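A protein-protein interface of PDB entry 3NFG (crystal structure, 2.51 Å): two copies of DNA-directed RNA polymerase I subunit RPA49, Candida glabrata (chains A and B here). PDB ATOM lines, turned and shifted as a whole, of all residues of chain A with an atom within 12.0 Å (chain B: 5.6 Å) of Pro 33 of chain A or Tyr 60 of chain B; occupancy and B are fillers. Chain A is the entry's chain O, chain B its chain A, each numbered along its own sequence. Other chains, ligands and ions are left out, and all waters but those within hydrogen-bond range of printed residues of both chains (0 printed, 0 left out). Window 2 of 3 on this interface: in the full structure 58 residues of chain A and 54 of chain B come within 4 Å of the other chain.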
ATOM      1  N   VAL A  22      -9.364 -11.927   8.588  1.00  0.00           N
ATOM      2  CA  VAL A  22     -10.036 -12.842   9.516  1.00  0.00           C
ATOM      3  C   VAL A  22      -9.149 -13.069  10.724  1.00  0.00           C
ATOM      4  O   VAL A  22      -7.955 -13.296  10.568  1.00  0.00           O
ATOM      5  CB  VAL A  22     -10.475 -14.184   8.866  1.00  0.00           C
ATOM      6  CG1 VAL A  22     -11.181 -15.084   9.876  1.00  0.00           C
ATOM      7  CG2 VAL A  22     -11.385 -13.944   7.671  1.00  0.00           C
ATOM      8  N   VAL A  23      -9.715 -12.976  11.927  1.00  0.00           N
ATOM      9  CA  VAL A  23      -8.953 -13.241  13.141  1.00  0.00           C
ATOM     10  C   VAL A  23      -9.412 -14.638  13.579  1.00  0.00           C
ATOM     11  O   VAL A  23     -10.595 -14.849  13.911  1.00  0.00           O
ATOM     12  CB  VAL A  23      -9.139 -12.159  14.239  1.00  0.00           C
ATOM     13  CG1 VAL A  23      -8.428 -12.540  15.529  1.00  0.00           C
ATOM     14  CG2 VAL A  23      -8.678 -10.794  13.754  1.00  0.00           C
ATOM     15  N   SER A  24      -8.500 -15.611  13.482  1.00  0.00           N
ATOM     16  CA  SER A  24      -8.833 -16.978  13.896  1.00  0.00           C
ATOM     17  C   SER A  24      -8.359 -17.216  15.303  1.00  0.00           C
ATOM     18  O   SER A  24      -7.329 -16.683  15.699  1.00  0.00           O
ATOM     19  CB  SER A  24      -8.251 -18.021  12.951  1.00  0.00           C
ATOM     20  OG  SER A  24      -8.900 -19.265  13.173  1.00  0.00           O
ATOM     21  N   ASN A  25      -9.125 -17.971  16.071  1.00  0.00           N
ATOM     22  CA  ASN A  25      -8.778 -18.281  17.442  1.00  0.00           C
ATOM     23  C   ASN A  25      -8.623 -19.796  17.616  1.00  0.00           C
ATOM     24  O   ASN A  25      -9.602 -20.542  17.532  1.00  0.00           O
ATOM     25  CB  ASN A  25      -9.810 -17.687  18.411  1.00  0.00           C
ATOM     26  CG  ASN A  25      -9.581 -18.056  19.861  1.00  0.00           C
ATOM     27  OD1 ASN A  25      -8.438 -18.142  20.350  1.00  0.00           O
ATOM     28  ND2 ASN A  25     -10.678 -18.263  20.586  1.00  0.00           N
ATOM     29  N   PHE A  26      -7.383 -20.250  17.809  1.00  0.00           N
ATOM     30  CA  PHE A  26      -7.095 -21.662  18.038  1.00  0.00           C
ATOM     31  C   PHE A  26      -6.764 -21.849  19.531  1.00  0.00           C
ATOM     32  O   PHE A  26      -7.641 -21.710  20.388  1.00  0.00           O
ATOM     33  CB  PHE A  26      -5.950 -22.147  17.133  1.00  0.00           C
ATOM     34  CG  PHE A  26      -6.222 -22.068  15.653  1.00  0.00           C
ATOM     35  CD1 PHE A  26      -6.872 -23.102  14.993  1.00  0.00           C
ATOM     36  CD2 PHE A  26      -5.791 -20.978  14.911  1.00  0.00           C
ATOM     37  CE1 PHE A  26      -7.086 -23.047  13.613  1.00  0.00           C
ATOM     38  CE2 PHE A  26      -6.016 -20.917  13.533  1.00  0.00           C
ATOM     39  CZ  PHE A  26      -6.674 -21.945  12.894  1.00  0.00           C
ATOM     40  N   PHE A  27      -5.492 -22.094  19.833  1.00  0.00           N
ATOM     41  CA  PHE A  27      -4.961 -22.280  21.181  1.00  0.00           C
ATOM     42  C   PHE A  27      -3.618 -21.559  21.261  1.00  0.00           C
ATOM     43  O   PHE A  27      -3.025 -21.268  20.214  1.00  0.00           O
ATOM     44  CB  PHE A  27      -4.787 -23.776  21.462  1.00  0.00           C
ATOM     45  CG  PHE A  27      -3.998 -24.500  20.401  1.00  0.00           C
ATOM     46  CD1 PHE A  27      -2.616 -24.614  20.495  1.00  0.00           C
ATOM     47  CD2 PHE A  27      -4.635 -25.068  19.300  1.00  0.00           C
ATOM     48  CE1 PHE A  27      -1.887 -25.279  19.511  1.00  0.00           C
ATOM     49  CE2 PHE A  27      -3.903 -25.730  18.311  1.00  0.00           C
ATOM     50  CZ  PHE A  27      -2.537 -25.835  18.426  1.00  0.00           C
ATOM     51  N   GLY A  29       0.099 -20.790  21.285  1.00  0.00           N
ATOM     52  CA  GLY A  29       1.257 -21.410  20.656  1.00  0.00           C
ATOM     53  C   GLY A  29       0.989 -22.157  19.364  1.00  0.00           C
ATOM     54  O   GLY A  29       1.830 -22.948  18.919  1.00  0.00           O
ATOM     55  N   VAL A  30      -0.180 -21.924  18.758  1.00  0.00           N
ATOM     56  CA  VAL A  30      -0.578 -22.562  17.501  1.00  0.00           C
ATOM     57  C   VAL A  30       0.467 -22.351  16.384  1.00  0.00           C
ATOM     58  O   VAL A  30       1.101 -21.297  16.304  1.00  0.00           O
ATOM     59  CB  VAL A  30      -2.041 -22.162  17.094  1.00  0.00           C
ATOM     60  CG1 VAL A  30      -2.175 -20.668  16.860  1.00  0.00           C
ATOM     61  CG2 VAL A  30      -2.551 -22.948  15.886  1.00  0.00           C
ATOM     62  N   ARG A  31       0.657 -23.371  15.561  1.00  0.00           N
ATOM     63  CA  ARG A  31       1.570 -23.310  14.429  1.00  0.00           C
ATOM     64  C   ARG A  31       0.806 -23.702  13.162  1.00  0.00           C
ATOM     65  O   ARG A  31       0.326 -24.838  13.043  1.00  0.00           O
ATOM     66  CB  ARG A  31       2.790 -24.233  14.645  1.00  0.00           C
ATOM     67  CG  ARG A  31       3.757 -23.812  15.752  1.00  0.00           C
ATOM     68  CD  ARG A  31       4.597 -24.976  16.262  1.00  0.00           C
ATOM     69  NE  ARG A  31       3.809 -25.873  17.110  1.00  0.00           N
ATOM     70  CZ  ARG A  31       4.149 -27.120  17.413  1.00  0.00           C
ATOM     71  NH1 ARG A  31       5.277 -27.643  16.948  1.00  0.00           N
ATOM     72  NH2 ARG A  31       3.361 -27.858  18.182  1.00  0.00           N
ATOM     73  N   VAL A  32       0.632 -22.749  12.249  1.00  0.00           N
ATOM     74  CA  VAL A  32      -0.073 -23.021  11.000  1.00  0.00           C
ATOM     75  C   VAL A  32       0.946 -22.952   9.861  1.00  0.00           C
ATOM     76  O   VAL A  32       1.589 -21.911   9.702  1.00  0.00           O
ATOM     77  CB  VAL A  32      -1.314 -22.107  10.769  1.00  0.00           C
ATOM     78  CG1 VAL A  32      -2.045 -22.478   9.478  1.00  0.00           C
ATOM     79  CG2 VAL A  32      -2.276 -22.149  11.966  1.00  0.00           C
ATOM     80  N   PRO A  33       1.136 -24.056   9.087  1.00  0.00           N
ATOM     81  CA  PRO A  33       2.121 -24.031   7.982  1.00  0.00           C
ATOM     82  C   PRO A  33       1.843 -22.917   6.973  1.00  0.00           C
ATOM     83  O   PRO A  33       0.677 -22.676   6.632  1.00  0.00           O
ATOM     84  CB  PRO A  33       1.973 -25.418   7.337  1.00  0.00           C
ATOM     85  CG  PRO A  33       1.357 -26.263   8.376  1.00  0.00           C
ATOM     86  CD  PRO A  33       0.459 -25.366   9.163  1.00  0.00           C
ATOM     87  N   LYS A  34       2.909 -22.222   6.520  1.00  0.00           N
ATOM     88  CA  LYS A  34       2.804 -21.097   5.572  1.00  0.00           C
ATOM     89  C   LYS A  34       2.059 -21.385   4.263  1.00  0.00           C
ATOM     90  O   LYS A  34       1.430 -20.481   3.707  1.00  0.00           O
ATOM     91  CB  LYS A  34       4.133 -20.326   5.380  1.00  0.00           C
ATOM     92  CG  LYS A  34       5.265 -21.070   4.685  1.00  0.00           C
ATOM     93  CD  LYS A  34       6.460 -20.164   4.475  1.00  0.00           C
ATOM     94  CE  LYS A  34       7.671 -20.956   4.050  1.00  0.00           C
ATOM     95  NZ  LYS A  34       8.900 -20.122   4.021  1.00  0.00           N
ATOM     96  N   ASP A  35       2.079 -22.659   3.818  1.00  0.00           N
ATOM     97  CA  ASP A  35       1.400 -23.158   2.617  1.00  0.00           C
ATOM     98  C   ASP A  35      -0.116 -23.300   2.765  1.00  0.00           C
ATOM     99  O   ASP A  35      -0.807 -23.308   1.740  1.00  0.00           O
ATOM    100  CB  ASP A  35       1.988 -24.516   2.185  1.00  0.00           C
ATOM    101  CG  ASP A  35       3.466 -24.523   1.880  1.00  0.00           C
ATOM    102  OD1 ASP A  35       3.996 -23.466   1.488  1.00  0.00           O
ATOM    103  OD2 ASP A  35       4.086 -25.597   1.994  1.00  0.00           O
ATOM    104  N   THR A  36      -0.632 -23.446   4.019  1.00  0.00           N
ATOM    105  CA  THR A  36      -2.068 -23.617   4.314  1.00  0.00           C
ATOM    106  C   THR A  36      -2.934 -22.528   3.692  1.00  0.00           C
ATOM    107  O   THR A  36      -2.707 -21.338   3.930  1.00  0.00           O
ATOM    108  CB  THR A  36      -2.347 -23.760   5.822  1.00  0.00           C
ATOM    109  OG1 THR A  36      -1.408 -24.660   6.412  1.00  0.00           O
ATOM    110  CG2 THR A  36      -3.753 -24.255   6.105  1.00  0.00           C
ATOM    111  N   GLU A  37      -3.920 -22.966   2.886  1.00  0.00           N
ATOM    112  CA  GLU A  37      -4.890 -22.119   2.190  1.00  0.00           C
ATOM    113  C   GLU A  37      -6.268 -22.227   2.850  1.00  0.00           C
ATOM    114  O   GLU A  37      -6.740 -23.333   3.121  1.00  0.00           O
ATOM    115  CB  GLU A  37      -4.970 -22.469   0.684  1.00  0.00           C
ATOM    116  CG  GLU A  37      -3.624 -22.480  -0.040  1.00  0.00           C
ATOM    117  CD  GLU A  37      -3.587 -22.089  -1.508  1.00  0.00           C
ATOM    118  OE1 GLU A  37      -4.602 -22.285  -2.219  1.00  0.00           O
ATOM    119  OE2 GLU A  37      -2.522 -21.597  -1.949  1.00  0.00           O
ATOM    120  N   PHE A  38      -6.896 -21.072   3.124  1.00  0.00           N
ATOM    121  CA  PHE A  38      -8.209 -20.969   3.769  1.00  0.00           C
ATOM    122  C   PHE A  38      -9.209 -20.267   2.872  1.00  0.00           C
ATOM    123  O   PHE A  38      -8.823 -19.435   2.048  1.00  0.00           O
ATOM    124  CB  PHE A  38      -8.107 -20.148   5.068  1.00  0.00           C
ATOM    125  CG  PHE A  38      -7.248 -20.702   6.174  1.00  0.00           C
ATOM    126  CD1 PHE A  38      -7.816 -21.385   7.238  1.00  0.00           C
ATOM    127  CD2 PHE A  38      -5.874 -20.477   6.188  1.00  0.00           C
ATOM    128  CE1 PHE A  38      -7.023 -21.880   8.275  1.00  0.00           C
ATOM    129  CE2 PHE A  38      -5.078 -20.974   7.226  1.00  0.00           C
ATOM    130  CZ  PHE A  38      -5.658 -21.674   8.263  1.00  0.00           C
ATOM    131  N   GLN A  39     -10.504 -20.554   3.087  1.00  0.00           N
ATOM    132  CA  GLN A  39     -11.631 -19.909   2.402  1.00  0.00           C
ATOM    133  C   GLN A  39     -12.591 -19.376   3.450  1.00  0.00           C
ATOM    134  O   GLN A  39     -12.737 -19.988   4.515  1.00  0.00           O
ATOM    135  CB  GLN A  39     -12.386 -20.882   1.483  1.00  0.00           C
ATOM    136  CG  GLN A  39     -11.677 -21.193   0.175  1.00  0.00           C
ATOM    137  CD  GLN A  39     -10.640 -22.256   0.342  1.00  0.00           C
ATOM    138  OE1 GLN A  39     -10.914 -23.345   0.859  1.00  0.00           O
ATOM    139  NE2 GLN A  39      -9.422 -21.951  -0.084  1.00  0.00           N
ATOM    140  N   LEU A  40     -13.253 -18.247   3.142  1.00  0.00           N
ATOM    141  CA  LEU A  40     -14.221 -17.622   4.034  1.00  0.00           C
ATOM    142  C   LEU A  40     -15.589 -17.716   3.425  1.00  0.00           C
ATOM    143  O   LEU A  40     -15.734 -17.526   2.229  1.00  0.00           O
ATOM    144  CB  LEU A  40     -13.827 -16.166   4.340  1.00  0.00           C
ATOM    145  CG  LEU A  40     -14.613 -15.448   5.428  1.00  0.00           C
ATOM    146  CD1 LEU A  40     -14.443 -16.107   6.766  1.00  0.00           C
ATOM    147  CD2 LEU A  40     -14.246 -14.001   5.474  1.00  0.00           C
ATOM    148  N   TYR A  41     -16.583 -18.050   4.245  1.00  0.00           N
ATOM    149  CA  TYR A  41     -17.979 -18.214   3.835  1.00  0.00           C
ATOM    150  C   TYR A  41     -18.848 -17.342   4.721  1.00  0.00           C
ATOM    151  O   TYR A  41     -18.662 -17.332   5.938  1.00  0.00           O
ATOM    152  CB  TYR A  41     -18.408 -19.697   3.916  1.00  0.00           C
ATOM    153  CG  TYR A  41     -17.521 -20.641   3.121  1.00  0.00           C
ATOM    154  CD1 TYR A  41     -17.853 -21.015   1.826  1.00  0.00           C
ATOM    155  CD2 TYR A  41     -16.365 -21.183   3.678  1.00  0.00           C
ATOM    156  CE1 TYR A  41     -17.044 -21.878   1.089  1.00  0.00           C
ATOM    157  CE2 TYR A  41     -15.537 -22.036   2.945  1.00  0.00           C
ATOM    158  CZ  TYR A  41     -15.880 -22.384   1.648  1.00  0.00           C
ATOM    159  OH  TYR A  41     -15.068 -23.241   0.929  1.00  0.00           O
ATOM    160  N   LEU B  51     -15.226 -20.514   8.568  1.00  0.00           N
ATOM    161  CA  LEU B  51     -13.872 -20.584   8.024  1.00  0.00           C
ATOM    162  C   LEU B  51     -13.459 -22.048   7.821  1.00  0.00           C
ATOM    163  O   LEU B  51     -13.554 -22.852   8.755  1.00  0.00           O
ATOM    164  CB  LEU B  51     -12.885 -19.857   8.957  1.00  0.00           C
ATOM    165  CG  LEU B  51     -11.404 -19.956   8.623  1.00  0.00           C
ATOM    166  CD1 LEU B  51     -11.041 -19.037   7.484  1.00  0.00           C
ATOM    167  CD2 LEU B  51     -10.560 -19.640   9.832  1.00  0.00           C
ATOM    168  N   HIS B  52     -13.015 -22.388   6.599  1.00  0.00           N
ATOM    169  CA  HIS B  52     -12.499 -23.718   6.278  1.00  0.00           C
ATOM    170  C   HIS B  52     -11.122 -23.620   5.633  1.00  0.00           C
ATOM    171  O   HIS B  52     -10.912 -22.820   4.715  1.00  0.00           O
ATOM    172  CB  HIS B  52     -13.457 -24.562   5.421  1.00  0.00           C
ATOM    173  CG  HIS B  52     -12.899 -25.918   5.093  1.00  0.00           C
ATOM    174  ND1 HIS B  52     -12.875 -26.938   6.031  1.00  0.00           N
ATOM    175  CD2 HIS B  52     -12.298 -26.356   3.961  1.00  0.00           C
ATOM    176  CE1 HIS B  52     -12.286 -27.964   5.435  1.00  0.00           C
ATOM    177  NE2 HIS B  52     -11.918 -27.661   4.189  1.00  0.00           N
ATOM    178  N   GLY B  53     -10.206 -24.435   6.152  1.00  0.00           N
ATOM    179  CA  GLY B  53      -8.829 -24.565   5.690  1.00  0.00           C
ATOM    180  C   GLY B  53      -8.465 -26.009   5.409  1.00  0.00           C
ATOM    181  O   GLY B  53      -9.181 -26.926   5.825  1.00  0.00           O
ATOM    182  N   GLU B  54      -7.345 -26.217   4.690  1.00  0.00           N
ATOM    183  CA  GLU B  54      -6.839 -27.542   4.320  1.00  0.00           C
ATOM    184  C   GLU B  54      -5.364 -27.497   3.874  1.00  0.00           C
ATOM    185  O   GLU B  54      -4.778 -26.423   3.708  1.00  0.00           O
ATOM    186  CB  GLU B  54      -7.723 -28.176   3.214  1.00  0.00           C
ATOM    187  CG  GLU B  54      -8.096 -29.631   3.471  1.00  0.00           C
ATOM    188  CD  GLU B  54      -8.981 -30.278   2.419  1.00  0.00           C
ATOM    189  OE1 GLU B  54     -10.199 -29.986   2.400  1.00  0.00           O
ATOM    190  OE2 GLU B  54      -8.460 -31.096   1.627  1.00  0.00           O
ATOM    191  N   ASN B  55      -4.782 -28.705   3.724  1.00  0.00           N
ATOM    192  CA  ASN B  55      -3.458 -29.137   3.246  1.00  0.00           C
ATOM    193  C   ASN B  55      -3.518 -30.676   3.246  1.00  0.00           C
ATOM    194  O   ASN B  55      -4.561 -31.229   3.606  1.00  0.00           O
ATOM    195  CB  ASN B  55      -2.260 -28.567   4.063  1.00  0.00           C
ATOM    196  CG  ASN B  55      -2.328 -28.694   5.570  1.00  0.00           C
ATOM    197  OD1 ASN B  55      -2.681 -27.746   6.276  1.00  0.00           O
ATOM    198  ND2 ASN B  55      -1.880 -29.816   6.106  1.00  0.00           N
ATOM    199  N   LEU B  58      -3.617 -31.776   7.540  1.00  0.00           N
ATOM    200  CA  LEU B  58      -4.639 -31.316   8.491  1.00  0.00           C
ATOM    201  C   LEU B  58      -5.842 -30.596   7.833  1.00  0.00           C
ATOM    202  O   LEU B  58      -5.761 -30.160   6.682  1.00  0.00           O
ATOM    203  CB  LEU B  58      -4.018 -30.396   9.574  1.00  0.00           C
ATOM    204  CG  LEU B  58      -2.805 -30.902  10.365  1.00  0.00           C
ATOM    205  CD1 LEU B  58      -2.069 -29.757  11.002  1.00  0.00           C
ATOM    206  CD2 LEU B  58      -3.198 -31.930  11.421  1.00  0.00           C
ATOM    207  N   GLU B  59      -6.957 -30.476   8.586  1.00  0.00           N
ATOM    208  CA  GLU B  59      -8.167 -29.751   8.193  1.00  0.00           C
ATOM    209  C   GLU B  59      -8.468 -28.709   9.274  1.00  0.00           C
ATOM    210  O   GLU B  59      -8.361 -29.016  10.465  1.00  0.00           O
ATOM    211  CB  GLU B  59      -9.360 -30.692   7.975  1.00  0.00           C
ATOM    212  CG  GLU B  59      -9.388 -31.293   6.577  1.00  0.00           C
ATOM    213  CD  GLU B  59     -10.728 -31.763   6.037  1.00  0.00           C
ATOM    214  OE1 GLU B  59     -11.781 -31.247   6.482  1.00  0.00           O
ATOM    215  OE2 GLU B  59     -10.720 -32.618   5.123  1.00  0.00           O
ATOM    216  N   TYR B  60      -8.794 -27.473   8.860  1.00  0.00           N
ATOM    217  CA  TYR B  60      -9.047 -26.340   9.750  1.00  0.00           C
ATOM    218  C   TYR B  60     -10.500 -25.911   9.599  1.00  0.00           C
ATOM    219  O   TYR B  60     -10.946 -25.660   8.478  1.00  0.00           O
ATOM    220  CB  TYR B  60      -8.089 -25.178   9.408  1.00  0.00           C
ATOM    221  CG  TYR B  60      -6.623 -25.546   9.492  1.00  0.00           C
ATOM    222  CD1 TYR B  60      -5.872 -25.244  10.622  1.00  0.00           C
ATOM    223  CD2 TYR B  60      -5.987 -26.207   8.443  1.00  0.00           C
ATOM    224  CE1 TYR B  60      -4.528 -25.600  10.715  1.00  0.00           C
ATOM    225  CE2 TYR B  60      -4.651 -26.594   8.535  1.00  0.00           C
ATOM    226  CZ  TYR B  60      -3.917 -26.269   9.665  1.00  0.00           C
ATOM    227  OH  TYR B  60      -2.590 -26.632   9.751  1.00  0.00           O
ATOM    228  N   ASP B  61     -11.253 -25.857  10.713  1.00  0.00           N
ATOM    229  CA  ASP B  61     -12.673 -25.497  10.688  1.00  0.00           C
ATOM    230  C   ASP B  61     -13.074 -24.615  11.864  1.00  0.00           C
ATOM    231  O   ASP B  61     -12.840 -24.986  13.010  1.00  0.00           O
ATOM    232  CB  ASP B  61     -13.552 -26.765  10.605  1.00  0.00           C
ATOM    233  CG  ASP B  61     -13.532 -27.439   9.239  1.00  0.00           C
ATOM    234  OD1 ASP B  61     -14.226 -26.945   8.324  1.00  0.00           O
ATOM    235  OD2 ASP B  61     -12.803 -28.444   9.080  1.00  0.00           O
ATOM    236  N   GLY B  62     -13.677 -23.463  11.566  1.00  0.00           N
ATOM    237  CA  GLY B  62     -14.127 -22.498  12.572  1.00  0.00           C
ATOM    238  C   GLY B  62     -15.331 -21.648  12.205  1.00  0.00           C
ATOM    239  O   GLY B  62     -15.677 -21.514  11.030  1.00  0.00           O
ATOM    240  N   LYS B  97     -10.935 -25.131  15.058  1.00  0.00           N
ATOM    241  CA  LYS B  97     -10.445 -26.438  15.478  1.00  0.00           C
ATOM    242  C   LYS B  97      -9.545 -27.026  14.386  1.00  0.00           C
ATOM    243  O   LYS B  97      -9.790 -26.821  13.189  1.00  0.00           O
ATOM    244  CB  LYS B  97     -11.611 -27.406  15.720  1.00  0.00           C
ATOM    245  CG  LYS B  97     -12.508 -27.092  16.910  1.00  0.00           C
ATOM    246  CD  LYS B  97     -13.569 -28.205  17.044  1.00  0.00           C
ATOM    247  CE  LYS B  97     -14.991 -27.744  17.297  1.00  0.00           C
ATOM    248  NZ  LYS B  97     -15.993 -28.707  16.755  1.00  0.00           N
ATOM    249  N   ILE B  98      -8.522 -27.792  14.802  1.00  0.00           N
ATOM    250  CA  ILE B  98      -7.633 -28.497  13.871  1.00  0.00           C
ATOM    251  C   ILE B  98      -7.885 -29.995  14.041  1.00  0.00           C
ATOM    252  O   ILE B  98      -7.926 -30.499  15.168  1.00  0.00           O
ATOM    253  CB  ILE B  98      -6.132 -28.108  13.976  1.00  0.00           C
ATOM    254  CG1 ILE B  98      -5.952 -26.573  13.975  1.00  0.00           C
ATOM    255  CG2 ILE B  98      -5.334 -28.749  12.831  1.00  0.00           C
ATOM    256  CD1 ILE B  98      -4.639 -26.043  14.476  1.00  0.00           C
ATOM    257  N   VAL B  99      -8.110 -30.688  12.917  1.00  0.00           N
ATOM    258  CA  VAL B  99      -8.407 -32.115  12.860  1.00  0.00           C
ATOM    259  C   VAL B  99      -7.498 -32.783  11.824  1.00  0.00           C
ATOM    260  O   VAL B  99      -7.374 -32.286  10.699  1.00  0.00           O
ATOM    261  CB  VAL B  99      -9.925 -32.334  12.602  1.00  0.00           C
ATOM    262  CG1 VAL B  99     -10.219 -33.669  11.922  1.00  0.00           C
ATOM    263  CG2 VAL B  99     -10.738 -32.176  13.888  1.00  0.00           C
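CD2 of Leu 51 of chain B touches OG of Ser 24 of chain A (3.7 Å). Phe 26 of chain A touches Tyr 60 of chain B (CE1 to CD1, 3.9 Å). Val 30 of chain A touches Ile 98 of chain B (CG2 to CD1, 3.99 Å). OH of Tyr 60 of chain B touches CD of Pro 33 of chain A, 3.4 Å away. Thr 36 of chain A touches Glu 54 of chain B. Leu 51 of chain B touches Phe 38 of chain A. CA of Phe 38 of chain A touches O of His 52 of chain B, 3.4 Å away. CD1 of Phe 38 of chain A touches CA of Gly 53 of chain B (3.7 Å). Tyr 60 of chain B touches Phe 38 of chain A. Leu 51 of chain B touches Gln 39 of chain A (CD1 to O, 3.5 Å).
Of chain B, only Tyr 60 comes within 4 Å of Pro 33 of chain A. His 52 of chain B touches just these residues of chain A: Phe 38 and Gln 39. Of chain A, only Glu 37 (3.5 Å) and Phe 38 (3.7 Å) come within 4 Å of Gly 53 of chain B. No residue of chain A comes within 4 Å of Glu 59 of chain B. No residue of chain A comes within 4 Å of Asp 61 of chain B. No residue of chain A comes within 4 Å of Gly 62 of chain B. Of the printed residues of chain B, Phe 27 of chain A touches Ile 98 (3.9 Å). Of the printed residues of chain A, Glu 54 of chain B touches Thr 36 and Glu 37. Of the printed residues of chain B, Phe 26 of chain A touches Tyr 60 and Ile 98. Asn 25 of chain A touches none of the printed residues of chain B. The nearest residue of chain A that does not touch Tyr 60 of chain B is Val 32 of chain A (4.2 Å).
The backbone carbonyl oxygen (O) of His 52 of chain B lies within hydrogen-bond range of the backbone NH (N) of Gln 39 of chain A (2.8 Å). N of Glu 54 of chain B is in hydrogen-bond range of O of Glu 37 of chain A (3.3 Å). The side-chain hydroxyl of Thr 36 of chain A sits at hydrogen-bond distance from the side-chain amide oxygen of Asn 55 of chain B (3.3 Å).
Of the 13 printed residues of chain B, 7 touch a printed residue of chain A. Hydrophobic or aromatic side chains of chain B within 4 Å of the printed part of chain A: Leu 51, Tyr 60 and Ile 98. Along chain B the printed residues that touch a printed residue of chain A span positions 51 to 98. Hydrophobic or aromatic side chains of chain A within 4 Å of the printed part of chain B: Phe 26, Phe 27, Val 30, Pro 33 and Phe 38.
The backbone NH (N) of Leu 51 of chain B is in hydrogen-bond range of the backbone carbonyl oxygen (O) of Gly 62 of chain B (2.7 Å). A ring nitrogen (NE2) of His 52 of chain B lies within hydrogen-bond range of the side-chain carboxylate of Glu 54 of chain B, 3.4 Å away. ND1 of His 52 of chain B is in hydrogen-bond range of OD1 of Asp 61 of chain B (2.7 Å). The backbone NH of Gly 53 of chain B sits at hydrogen-bond distance from the backbone carbonyl oxygen of Tyr 60 of chain B, at 2.7 Å. The side-chain amide nitrogen of Asn 55 of chain B lies close to the backbone NH of Leu 58 of chain B (3.0 Å). The backbone carbonyl oxygen of Pro 33 of chain A sits at hydrogen-bond distance from the side-chain hydroxyl of Thr 36 of chain A (2.9 Å).
No position is printed for both chains.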
